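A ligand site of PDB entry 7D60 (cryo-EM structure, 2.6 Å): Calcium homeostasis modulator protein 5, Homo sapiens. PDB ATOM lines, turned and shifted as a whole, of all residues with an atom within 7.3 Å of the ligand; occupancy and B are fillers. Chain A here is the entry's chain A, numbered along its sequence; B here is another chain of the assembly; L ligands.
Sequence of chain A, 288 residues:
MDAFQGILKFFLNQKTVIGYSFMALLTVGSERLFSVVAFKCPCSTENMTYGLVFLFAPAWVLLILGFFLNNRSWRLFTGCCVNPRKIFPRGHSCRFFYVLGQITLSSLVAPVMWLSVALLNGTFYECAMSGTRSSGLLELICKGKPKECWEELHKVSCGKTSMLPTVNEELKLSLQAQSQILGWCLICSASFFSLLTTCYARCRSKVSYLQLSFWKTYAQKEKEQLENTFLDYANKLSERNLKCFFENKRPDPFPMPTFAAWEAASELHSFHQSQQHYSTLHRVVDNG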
ATOM      1  N   LEU A  33     -29.062 -10.234  10.085  1.00  0.00           N
ATOM      2  CA  LEU A  33     -28.184 -10.193   8.930  1.00  0.00           C
ATOM      3  C   LEU A  33     -27.351  -8.929   8.909  1.00  0.00           C
ATOM      4  O   LEU A  33     -26.238  -8.925   8.362  1.00  0.00           O
ATOM      5  CB  LEU A  33     -29.015 -10.334   7.648  1.00  0.00           C
ATOM      6  CG  LEU A  33     -28.327 -10.541   6.294  1.00  0.00           C
ATOM      7  CD1 LEU A  33     -29.096 -11.565   5.495  1.00  0.00           C
ATOM      8  CD2 LEU A  33     -28.260  -9.239   5.524  1.00  0.00           C
ATOM      9  N   PHE A  34     -27.847  -7.842   9.513  1.00  0.00           N
ATOM     10  CA  PHE A  34     -27.085  -6.605   9.541  1.00  0.00           C
ATOM     11  C   PHE A  34     -26.076  -6.581  10.666  1.00  0.00           C
ATOM     12  O   PHE A  34     -24.978  -6.024  10.498  1.00  0.00           O
ATOM     13  CB  PHE A  34     -28.038  -5.409   9.696  1.00  0.00           C
ATOM     14  CG  PHE A  34     -28.455  -4.816   8.393  1.00  0.00           C
ATOM     15  CD1 PHE A  34     -27.593  -4.014   7.671  1.00  0.00           C
ATOM     16  CD2 PHE A  34     -29.726  -5.042   7.883  1.00  0.00           C
ATOM     17  CE1 PHE A  34     -27.968  -3.467   6.463  1.00  0.00           C
ATOM     18  CE2 PHE A  34     -30.114  -4.498   6.679  1.00  0.00           C
ATOM     19  CZ  PHE A  34     -29.238  -3.706   5.974  1.00  0.00           C
ATOM     20  N   VAL A  36     -24.580  -9.235  12.138  1.00  0.00           N
ATOM     21  CA  VAL A  36     -23.560 -10.273  12.027  1.00  0.00           C
ATOM     22  C   VAL A  36     -22.623 -10.007  10.858  1.00  0.00           C
ATOM     23  O   VAL A  36     -21.408 -10.081  10.999  1.00  0.00           O
ATOM     24  CB  VAL A  36     -24.253 -11.654  11.917  1.00  0.00           C
ATOM     25  CG1 VAL A  36     -23.337 -12.698  11.297  1.00  0.00           C
ATOM     26  CG2 VAL A  36     -24.741 -12.100  13.274  1.00  0.00           C
ATOM     27  N   VAL A  37     -23.178  -9.647   9.711  1.00  0.00           N
ATOM     28  CA  VAL A  37     -22.410  -9.631   8.468  1.00  0.00           C
ATOM     29  C   VAL A  37     -21.854  -8.252   8.167  1.00  0.00           C
ATOM     30  O   VAL A  37     -20.723  -8.112   7.692  1.00  0.00           O
ATOM     31  CB  VAL A  37     -23.302 -10.165   7.329  1.00  0.00           C
ATOM     32  CG1 VAL A  37     -22.506 -10.336   6.064  1.00  0.00           C
ATOM     33  CG2 VAL A  37     -23.930 -11.484   7.729  1.00  0.00           C
ATOM     34  N   ALA A  38     -22.610  -7.184   8.440  1.00  0.00           N
ATOM     35  CA  ALA A  38     -22.206  -5.844   8.025  1.00  0.00           C
ATOM     36  C   ALA A  38     -21.719  -4.962   9.162  1.00  0.00           C
ATOM     37  O   ALA A  38     -20.828  -4.146   8.956  1.00  0.00           O
ATOM     38  CB  ALA A  38     -23.368  -5.156   7.317  1.00  0.00           C
ATOM     39  N   PHE A  39     -22.288  -5.095  10.352  1.00  0.00           N
ATOM     40  CA  PHE A  39     -21.943  -4.189  11.451  1.00  0.00           C
ATOM     41  C   PHE A  39     -20.636  -4.624  12.092  1.00  0.00           C
ATOM     42  O   PHE A  39     -20.485  -5.771  12.514  1.00  0.00           O
ATOM     43  CB  PHE A  39     -23.063  -4.171  12.496  1.00  0.00           C
ATOM     44  CG  PHE A  39     -22.943  -3.072  13.498  1.00  0.00           C
ATOM     45  CD1 PHE A  39     -22.366  -3.298  14.730  1.00  0.00           C
ATOM     46  CD2 PHE A  39     -23.431  -1.809  13.227  1.00  0.00           C
ATOM     47  CE1 PHE A  39     -22.257  -2.294  15.661  1.00  0.00           C
ATOM     48  CE2 PHE A  39     -23.337  -0.797  14.163  1.00  0.00           C
ATOM     49  CZ  PHE A  39     -22.747  -1.039  15.376  1.00  0.00           C
ATOM     50  N   LYS A  40     -19.683  -3.698  12.150  1.00  0.00           N
ATOM     51  CA  LYS A  40     -18.487  -3.865  12.970  1.00  0.00           C
ATOM     52  C   LYS A  40     -18.067  -2.489  13.462  1.00  0.00           C
ATOM     53  O   LYS A  40     -17.696  -1.619  12.681  1.00  0.00           O
ATOM     54  CB  LYS A  40     -17.367  -4.567  12.205  1.00  0.00           C
ATOM     55  CG  LYS A  40     -17.145  -4.130  10.770  1.00  0.00           C
ATOM     56  CD  LYS A  40     -16.126  -5.019  10.087  1.00  0.00           C
ATOM     57  CE  LYS A  40     -16.702  -6.393   9.810  1.00  0.00           C
ATOM     58  NZ  LYS A  40     -17.800  -6.343   8.813  1.00  0.00           N
ATOM     59  N   ALA B  24     -33.251  -5.816  -6.532  1.00  0.00           N
ATOM     60  CA  ALA B  24     -32.350  -5.604  -5.405  1.00  0.00           C
ATOM     61  C   ALA B  24     -31.595  -6.869  -5.058  1.00  0.00           C
ATOM     62  O   ALA B  24     -30.449  -6.798  -4.589  1.00  0.00           O
ATOM     63  CB  ALA B  24     -33.131  -5.099  -4.193  1.00  0.00           C
ATOM     64  N   LEU B  25     -32.202  -8.042  -5.265  1.00  0.00           N
ATOM     65  CA  LEU B  25     -31.518  -9.289  -4.977  1.00  0.00           C
ATOM     66  C   LEU B  25     -30.468  -9.610  -6.039  1.00  0.00           C
ATOM     67  O   LEU B  25     -29.506 -10.328  -5.747  1.00  0.00           O
ATOM     68  CB  LEU B  25     -32.547 -10.421  -4.851  1.00  0.00           C
ATOM     69  CG  LEU B  25     -32.165 -11.802  -4.315  1.00  0.00           C
ATOM     70  CD1 LEU B  25     -33.336 -12.362  -3.528  1.00  0.00           C
ATOM     71  CD2 LEU B  25     -31.794 -12.776  -5.428  1.00  0.00           C
ATOM     72  N   VAL B  28     -27.355  -7.129  -5.194  1.00  0.00           N
ATOM     73  CA  VAL B  28     -26.557  -7.547  -4.040  1.00  0.00           C
ATOM     74  C   VAL B  28     -25.667  -8.726  -4.413  1.00  0.00           C
ATOM     75  O   VAL B  28     -24.469  -8.740  -4.106  1.00  0.00           O
ATOM     76  CB  VAL B  28     -27.487  -7.874  -2.856  1.00  0.00           C
ATOM     77  CG1 VAL B  28     -26.758  -8.668  -1.792  1.00  0.00           C
ATOM     78  CG2 VAL B  28     -28.045  -6.591  -2.270  1.00  0.00           C
ATOM     79  N   GLY B  29     -26.234  -9.713  -5.105  1.00  0.00           N
ATOM     80  CA  GLY B  29     -25.462 -10.887  -5.494  1.00  0.00           C
ATOM     81  C   GLY B  29     -24.428 -10.639  -6.568  1.00  0.00           C
ATOM     82  O   GLY B  29     -23.505 -11.453  -6.722  1.00  0.00           O
ATOM     83  N   GLU B  31     -22.674  -7.626  -6.651  1.00  0.00           N
ATOM     84  CA  GLU B  31     -21.609  -6.875  -6.011  1.00  0.00           C
ATOM     85  C   GLU B  31     -20.704  -7.777  -5.184  1.00  0.00           C
ATOM     86  O   GLU B  31     -19.505  -7.505  -5.063  1.00  0.00           O
ATOM     87  CB  GLU B  31     -22.208  -5.776  -5.124  1.00  0.00           C
ATOM     88  CG  GLU B  31     -21.240  -4.667  -4.790  1.00  0.00           C
ATOM     89  CD  GLU B  31     -20.507  -4.908  -3.487  1.00  0.00           C
ATOM     90  OE1 GLU B  31     -20.982  -5.726  -2.671  1.00  0.00           O
ATOM     91  OE2 GLU B  31     -19.436  -4.297  -3.287  1.00  0.00           O
ATOM     92  N   ARG B  32     -21.244  -8.851  -4.606  1.00  0.00           N
ATOM     93  CA  ARG B  32     -20.416  -9.785  -3.863  1.00  0.00           C
ATOM     94  C   ARG B  32     -19.569 -10.652  -4.775  1.00  0.00           C
ATOM     95  O   ARG B  32     -18.596 -11.247  -4.315  1.00  0.00           O
ATOM     96  CB  ARG B  32     -21.291 -10.679  -2.982  1.00  0.00           C
ATOM     97  CG  ARG B  32     -22.155  -9.902  -2.027  1.00  0.00           C
ATOM     98  CD  ARG B  32     -21.302  -9.085  -1.084  1.00  0.00           C
ATOM     99  NE  ARG B  32     -20.339  -9.923  -0.388  1.00  0.00           N
ATOM    100  CZ  ARG B  32     -19.072  -9.588  -0.193  1.00  0.00           C
ATOM    101  NH1 ARG B  32     -18.608  -8.429  -0.646  1.00  0.00           N
ATOM    102  NH2 ARG B  32     -18.253 -10.411   0.450  1.00  0.00           N
ATOM    103  N   SER B  35     -16.473  -8.038  -5.672  1.00  0.00           N
ATOM    104  CA  SER B  35     -15.572  -7.680  -4.586  1.00  0.00           C
ATOM    105  C   SER B  35     -14.798  -8.863  -4.038  1.00  0.00           C
ATOM    106  O   SER B  35     -13.741  -8.659  -3.430  1.00  0.00           O
ATOM    107  CB  SER B  35     -16.377  -7.037  -3.452  1.00  0.00           C
ATOM    108  OG  SER B  35     -16.942  -8.032  -2.617  1.00  0.00           O
ATOM    109  N   VAL B  36     -15.277 -10.079  -4.242  1.00  0.00           N
ATOM    110  CA  VAL B  36     -14.587 -11.258  -3.751  1.00  0.00           C
ATOM    111  C   VAL B  36     -13.651 -11.831  -4.799  1.00  0.00           C
ATOM    112  O   VAL B  36     -12.496 -12.144  -4.518  1.00  0.00           O
ATOM    113  CB  VAL B  36     -15.632 -12.301  -3.282  1.00  0.00           C
ATOM    114  CG1 VAL B  36     -15.058 -13.707  -3.246  1.00  0.00           C
ATOM    115  CG2 VAL B  36     -16.187 -11.913  -1.923  1.00  0.00           C
ATOM    116  N   SER B 116     -25.459   2.003  -3.587  1.00  0.00           N
ATOM    117  CA  SER B 116     -25.757   1.822  -2.177  1.00  0.00           C
ATOM    118  C   SER B 116     -25.230   0.502  -1.642  1.00  0.00           C
ATOM    119  O   SER B 116     -24.712   0.456  -0.534  1.00  0.00           O
ATOM    120  CB  SER B 116     -27.262   1.903  -1.968  1.00  0.00           C
ATOM    121  OG  SER B 116     -27.742   3.195  -2.298  1.00  0.00           O
ATOM    122  N   VAL B 117     -25.364  -0.575  -2.416  1.00  0.00           N
ATOM    123  CA  VAL B 117     -24.827  -1.861  -1.984  1.00  0.00           C
ATOM    124  C   VAL B 117     -23.305  -1.852  -2.074  1.00  0.00           C
ATOM    125  O   VAL B 117     -22.634  -2.493  -1.255  1.00  0.00           O
ATOM    126  CB  VAL B 117     -25.462  -2.981  -2.844  1.00  0.00           C
ATOM    127  CG1 VAL B 117     -24.966  -4.362  -2.430  1.00  0.00           C
ATOM    128  CG2 VAL B 117     -26.960  -2.931  -2.706  1.00  0.00           C
ATOM    129  N   ALA B 118     -22.732  -1.097  -3.011  1.00  0.00           N
ATOM    130  CA  ALA B 118     -21.284  -1.007  -3.102  1.00  0.00           C
ATOM    131  C   ALA B 118     -20.691  -0.168  -1.985  1.00  0.00           C
ATOM    132  O   ALA B 118     -19.539  -0.370  -1.613  1.00  0.00           O
ATOM    133  CB  ALA B 118     -20.884  -0.451  -4.462  1.00  0.00           C
ATOM    134  N   LEU B 120     -22.223   0.054   1.109  1.00  0.00           N
ATOM    135  CA  LEU B 120     -22.462  -0.678   2.349  1.00  0.00           C
ATOM    136  C   LEU B 120     -21.513  -1.842   2.522  1.00  0.00           C
ATOM    137  O   LEU B 120     -21.448  -2.420   3.612  1.00  0.00           O
ATOM    138  CB  LEU B 120     -23.896  -1.180   2.412  1.00  0.00           C
ATOM    139  CG  LEU B 120     -25.030  -0.201   2.715  1.00  0.00           C
ATOM    140  CD1 LEU B 120     -26.316  -0.954   2.937  1.00  0.00           C
ATOM    141  CD2 LEU B 120     -24.702   0.661   3.911  1.00  0.00           C
ATOM    142  N   ASN B 121     -20.790  -2.223   1.477  1.00  0.00           N
ATOM    143  CA  ASN B 121     -19.733  -3.234   1.519  1.00  0.00           C
ATOM    144  C   ASN B 121     -18.466  -2.441   1.202  1.00  0.00           C
ATOM    145  O   ASN B 121     -18.083  -2.318   0.036  1.00  0.00           O
ATOM    146  CB  ASN B 121     -20.016  -4.358   0.527  1.00  0.00           C
ATOM    147  CG  ASN B 121     -18.825  -5.268   0.316  1.00  0.00           C
ATOM    148  OD1 ASN B 121     -18.631  -6.224   1.065  1.00  0.00           O
ATOM    149  ND2 ASN B 121     -18.036  -4.990  -0.713  1.00  0.00           N
ATOM    150  N   GLY B 122     -17.836  -1.902   2.234  1.00  0.00           N
ATOM    151  CA  GLY B 122     -16.907  -0.808   2.046  1.00  0.00           C
ATOM    152  C   GLY B 122     -15.520  -1.111   1.507  1.00  0.00           C
ATOM    153  O   GLY B 122     -14.542  -0.572   2.023  1.00  0.00           O
ATOM    154  N   THR B 123     -15.419  -1.929   0.462  1.00  0.00           N
ATOM    155  CA  THR B 123     -14.120  -2.242  -0.104  1.00  0.00           C
ATOM    156  C   THR B 123     -13.714  -1.297  -1.221  1.00  0.00           C
ATOM    157  O   THR B 123     -12.520  -1.040  -1.395  1.00  0.00           O
ATOM    158  CB  THR B 123     -14.101  -3.672  -0.632  1.00  0.00           C
ATOM    159  OG1 THR B 123     -15.026  -3.801  -1.709  1.00  0.00           O
ATOM    160  CG2 THR B 123     -14.503  -4.634   0.461  1.00  0.00           C
ATOM    161  N   GLN B 176     -13.793   1.890   6.616  1.00  0.00           N
ATOM    162  CA  GLN B 176     -14.912   1.007   6.337  1.00  0.00           C
ATOM    163  C   GLN B 176     -16.197   1.474   6.999  1.00  0.00           C
ATOM    164  O   GLN B 176     -17.282   1.038   6.595  1.00  0.00           O
ATOM    165  CB  GLN B 176     -14.545  -0.409   6.801  1.00  0.00           C
ATOM    166  CG  GLN B 176     -15.335  -1.551   6.198  1.00  0.00           C
ATOM    167  CD  GLN B 176     -16.335  -2.139   7.177  1.00  0.00           C
ATOM    168  OE1 GLN B 176     -16.257  -1.914   8.375  1.00  0.00           O
ATOM    169  NE2 GLN B 176     -17.279  -2.917   6.655  1.00  0.00           N
ATOM    170  N   GLN B 180     -20.002   3.226   5.053  1.00  0.00           N
ATOM    171  CA  GLN B 180     -21.315   2.717   5.413  1.00  0.00           C
ATOM    172  C   GLN B 180     -22.249   3.815   5.895  1.00  0.00           C
ATOM    173  O   GLN B 180     -23.466   3.630   5.875  1.00  0.00           O
ATOM    174  CB  GLN B 180     -21.177   1.625   6.464  1.00  0.00           C
ATOM    175  CG  GLN B 180     -20.604   0.350   5.911  1.00  0.00           C
ATOM    176  CD  GLN B 180     -20.520  -0.737   6.933  1.00  0.00           C
ATOM    177  OE1 GLN B 180     -20.220  -0.494   8.083  1.00  0.00           O
ATOM    178  NE2 GLN B 180     -20.801  -1.958   6.501  1.00  0.00           N
ATOM    179  N   TRP B 184     -25.933   4.820   3.798  1.00  0.00           N
ATOM    180  CA  TRP B 184     -27.262   5.057   4.367  1.00  0.00           C
ATOM    181  C   TRP B 184     -27.772   6.452   4.076  1.00  0.00           C
ATOM    182  O   TRP B 184     -28.991   6.659   4.086  1.00  0.00           O
ATOM    183  CB  TRP B 184     -27.254   4.817   5.875  1.00  0.00           C
ATOM    184  CG  TRP B 184     -27.242   3.387   6.280  1.00  0.00           C
ATOM    185  CD1 TRP B 184     -26.255   2.739   6.946  1.00  0.00           C
ATOM    186  CD2 TRP B 184     -28.260   2.412   6.037  1.00  0.00           C
ATOM    187  NE1 TRP B 184     -26.584   1.427   7.142  1.00  0.00           N
ATOM    188  CE2 TRP B 184     -27.821   1.199   6.592  1.00  0.00           C
ATOM    189  CE3 TRP B 184     -29.506   2.438   5.406  1.00  0.00           C
ATOM    190  CZ2 TRP B 184     -28.568   0.030   6.529  1.00  0.00           C
ATOM    191  CZ3 TRP B 184     -30.246   1.288   5.350  1.00  0.00           C
ATOM    192  CH2 TRP B 184     -29.775   0.101   5.904  1.00  0.00           C
HETATM  193  O1  LIG L   1     -18.129  -8.529   6.253  1.00  0.00           O
HETATM  194  O2  LIG L   1     -18.390  -6.380   5.067  1.00  0.00           O
HETATM  195  P1  LIG L   1     -18.262  -7.879   4.908  1.00  0.00           P
HETATM  196  O3  LIG L   1     -17.036  -8.192   4.083  1.00  0.00           O
HETATM  197  O4  LIG L   1     -19.607  -8.454   4.149  1.00  0.00           O
HETATM  198  C1  LIG L   1     -20.475  -7.523   3.558  1.00  0.00           C
HETATM  199  C2  LIG L   1     -21.764  -8.229   3.127  1.00  0.00           C
HETATM  200  C3  LIG L   1     -22.703  -7.175   2.522  1.00  0.00           C
HETATM  201  O5  LIG L   1     -24.011  -7.368   2.970  1.00  0.00           O
HETATM  202  C4  LIG L   1     -24.951  -6.527   2.356  1.00  0.00           C
HETATM  203  O6  LIG L   1     -24.598  -5.693   1.593  1.00  0.00           O
HETATM  204  C5  LIG L   1     -26.442  -6.650   2.672  1.00  0.00           C
HETATM  205  C6  LIG L   1     -27.185  -5.371   2.300  1.00  0.00           C
HETATM  206  C7  LIG L   1     -28.658  -5.607   1.966  1.00  0.00           C
HETATM  207  O7  LIG L   1     -21.465  -9.200   2.161  1.00  0.00           O
HETATM  208  C8  LIG L   1     -21.565 -10.545   2.567  1.00  0.00           C
HETATM  209  O8  LIG L   1     -20.775 -10.989   3.329  1.00  0.00           O
HETATM  210  C9  LIG L   1     -22.669 -11.435   2.017  1.00  0.00           C
HETATM  211  C10 LIG L   1     -23.997 -11.269   2.757  1.00  0.00           C
HETATM  212  C11 LIG L   1     -25.089 -10.690   1.857  1.00  0.00           C
HETATM  213  C12 LIG L   1     -26.480 -10.893   2.455  1.00  0.00           C
HETATM  214  C13 LIG L   1     -27.090 -12.252   2.093  1.00  0.00           C
HETATM  215  C14 LIG L   1     -28.306 -12.108   1.189  1.00  0.00           C
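NE of Arg 32 of chain B is in hydrogen-bond range of O7 of the ligand (2.9 Å).
The backbone carbonyl oxygen (O) of Val 37 sits close to an oxygen (O1) of the ligand, 3.0 Å away.
The side-chain amino group of Lys 40 is in salt-bridge range of an oxygen (O1) of the ligand, at 3.4 Å.
Leu 33 touches the ligand.
Asn 121 of chain B touches the ligand (OD1 to C1, 3.4 Å).
NE2 of Gln 176 of chain B touches O2 of the ligand, at 3.97 Å.
Hydrophobic or aromatic side chains within 4 Å of the ligand: Leu 33 and Val 37.
Within 4 Å of the ligand: Leu 33, Val 37, Lys 40, Arg 32 of chain B, Asn 121 of chain B and Gln 176 of chain B.
NH1 of Arg 32 of chain B sits at hydrogen-bond distance from OD1 of Asn 121 of chain B, at 2.8 Å.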
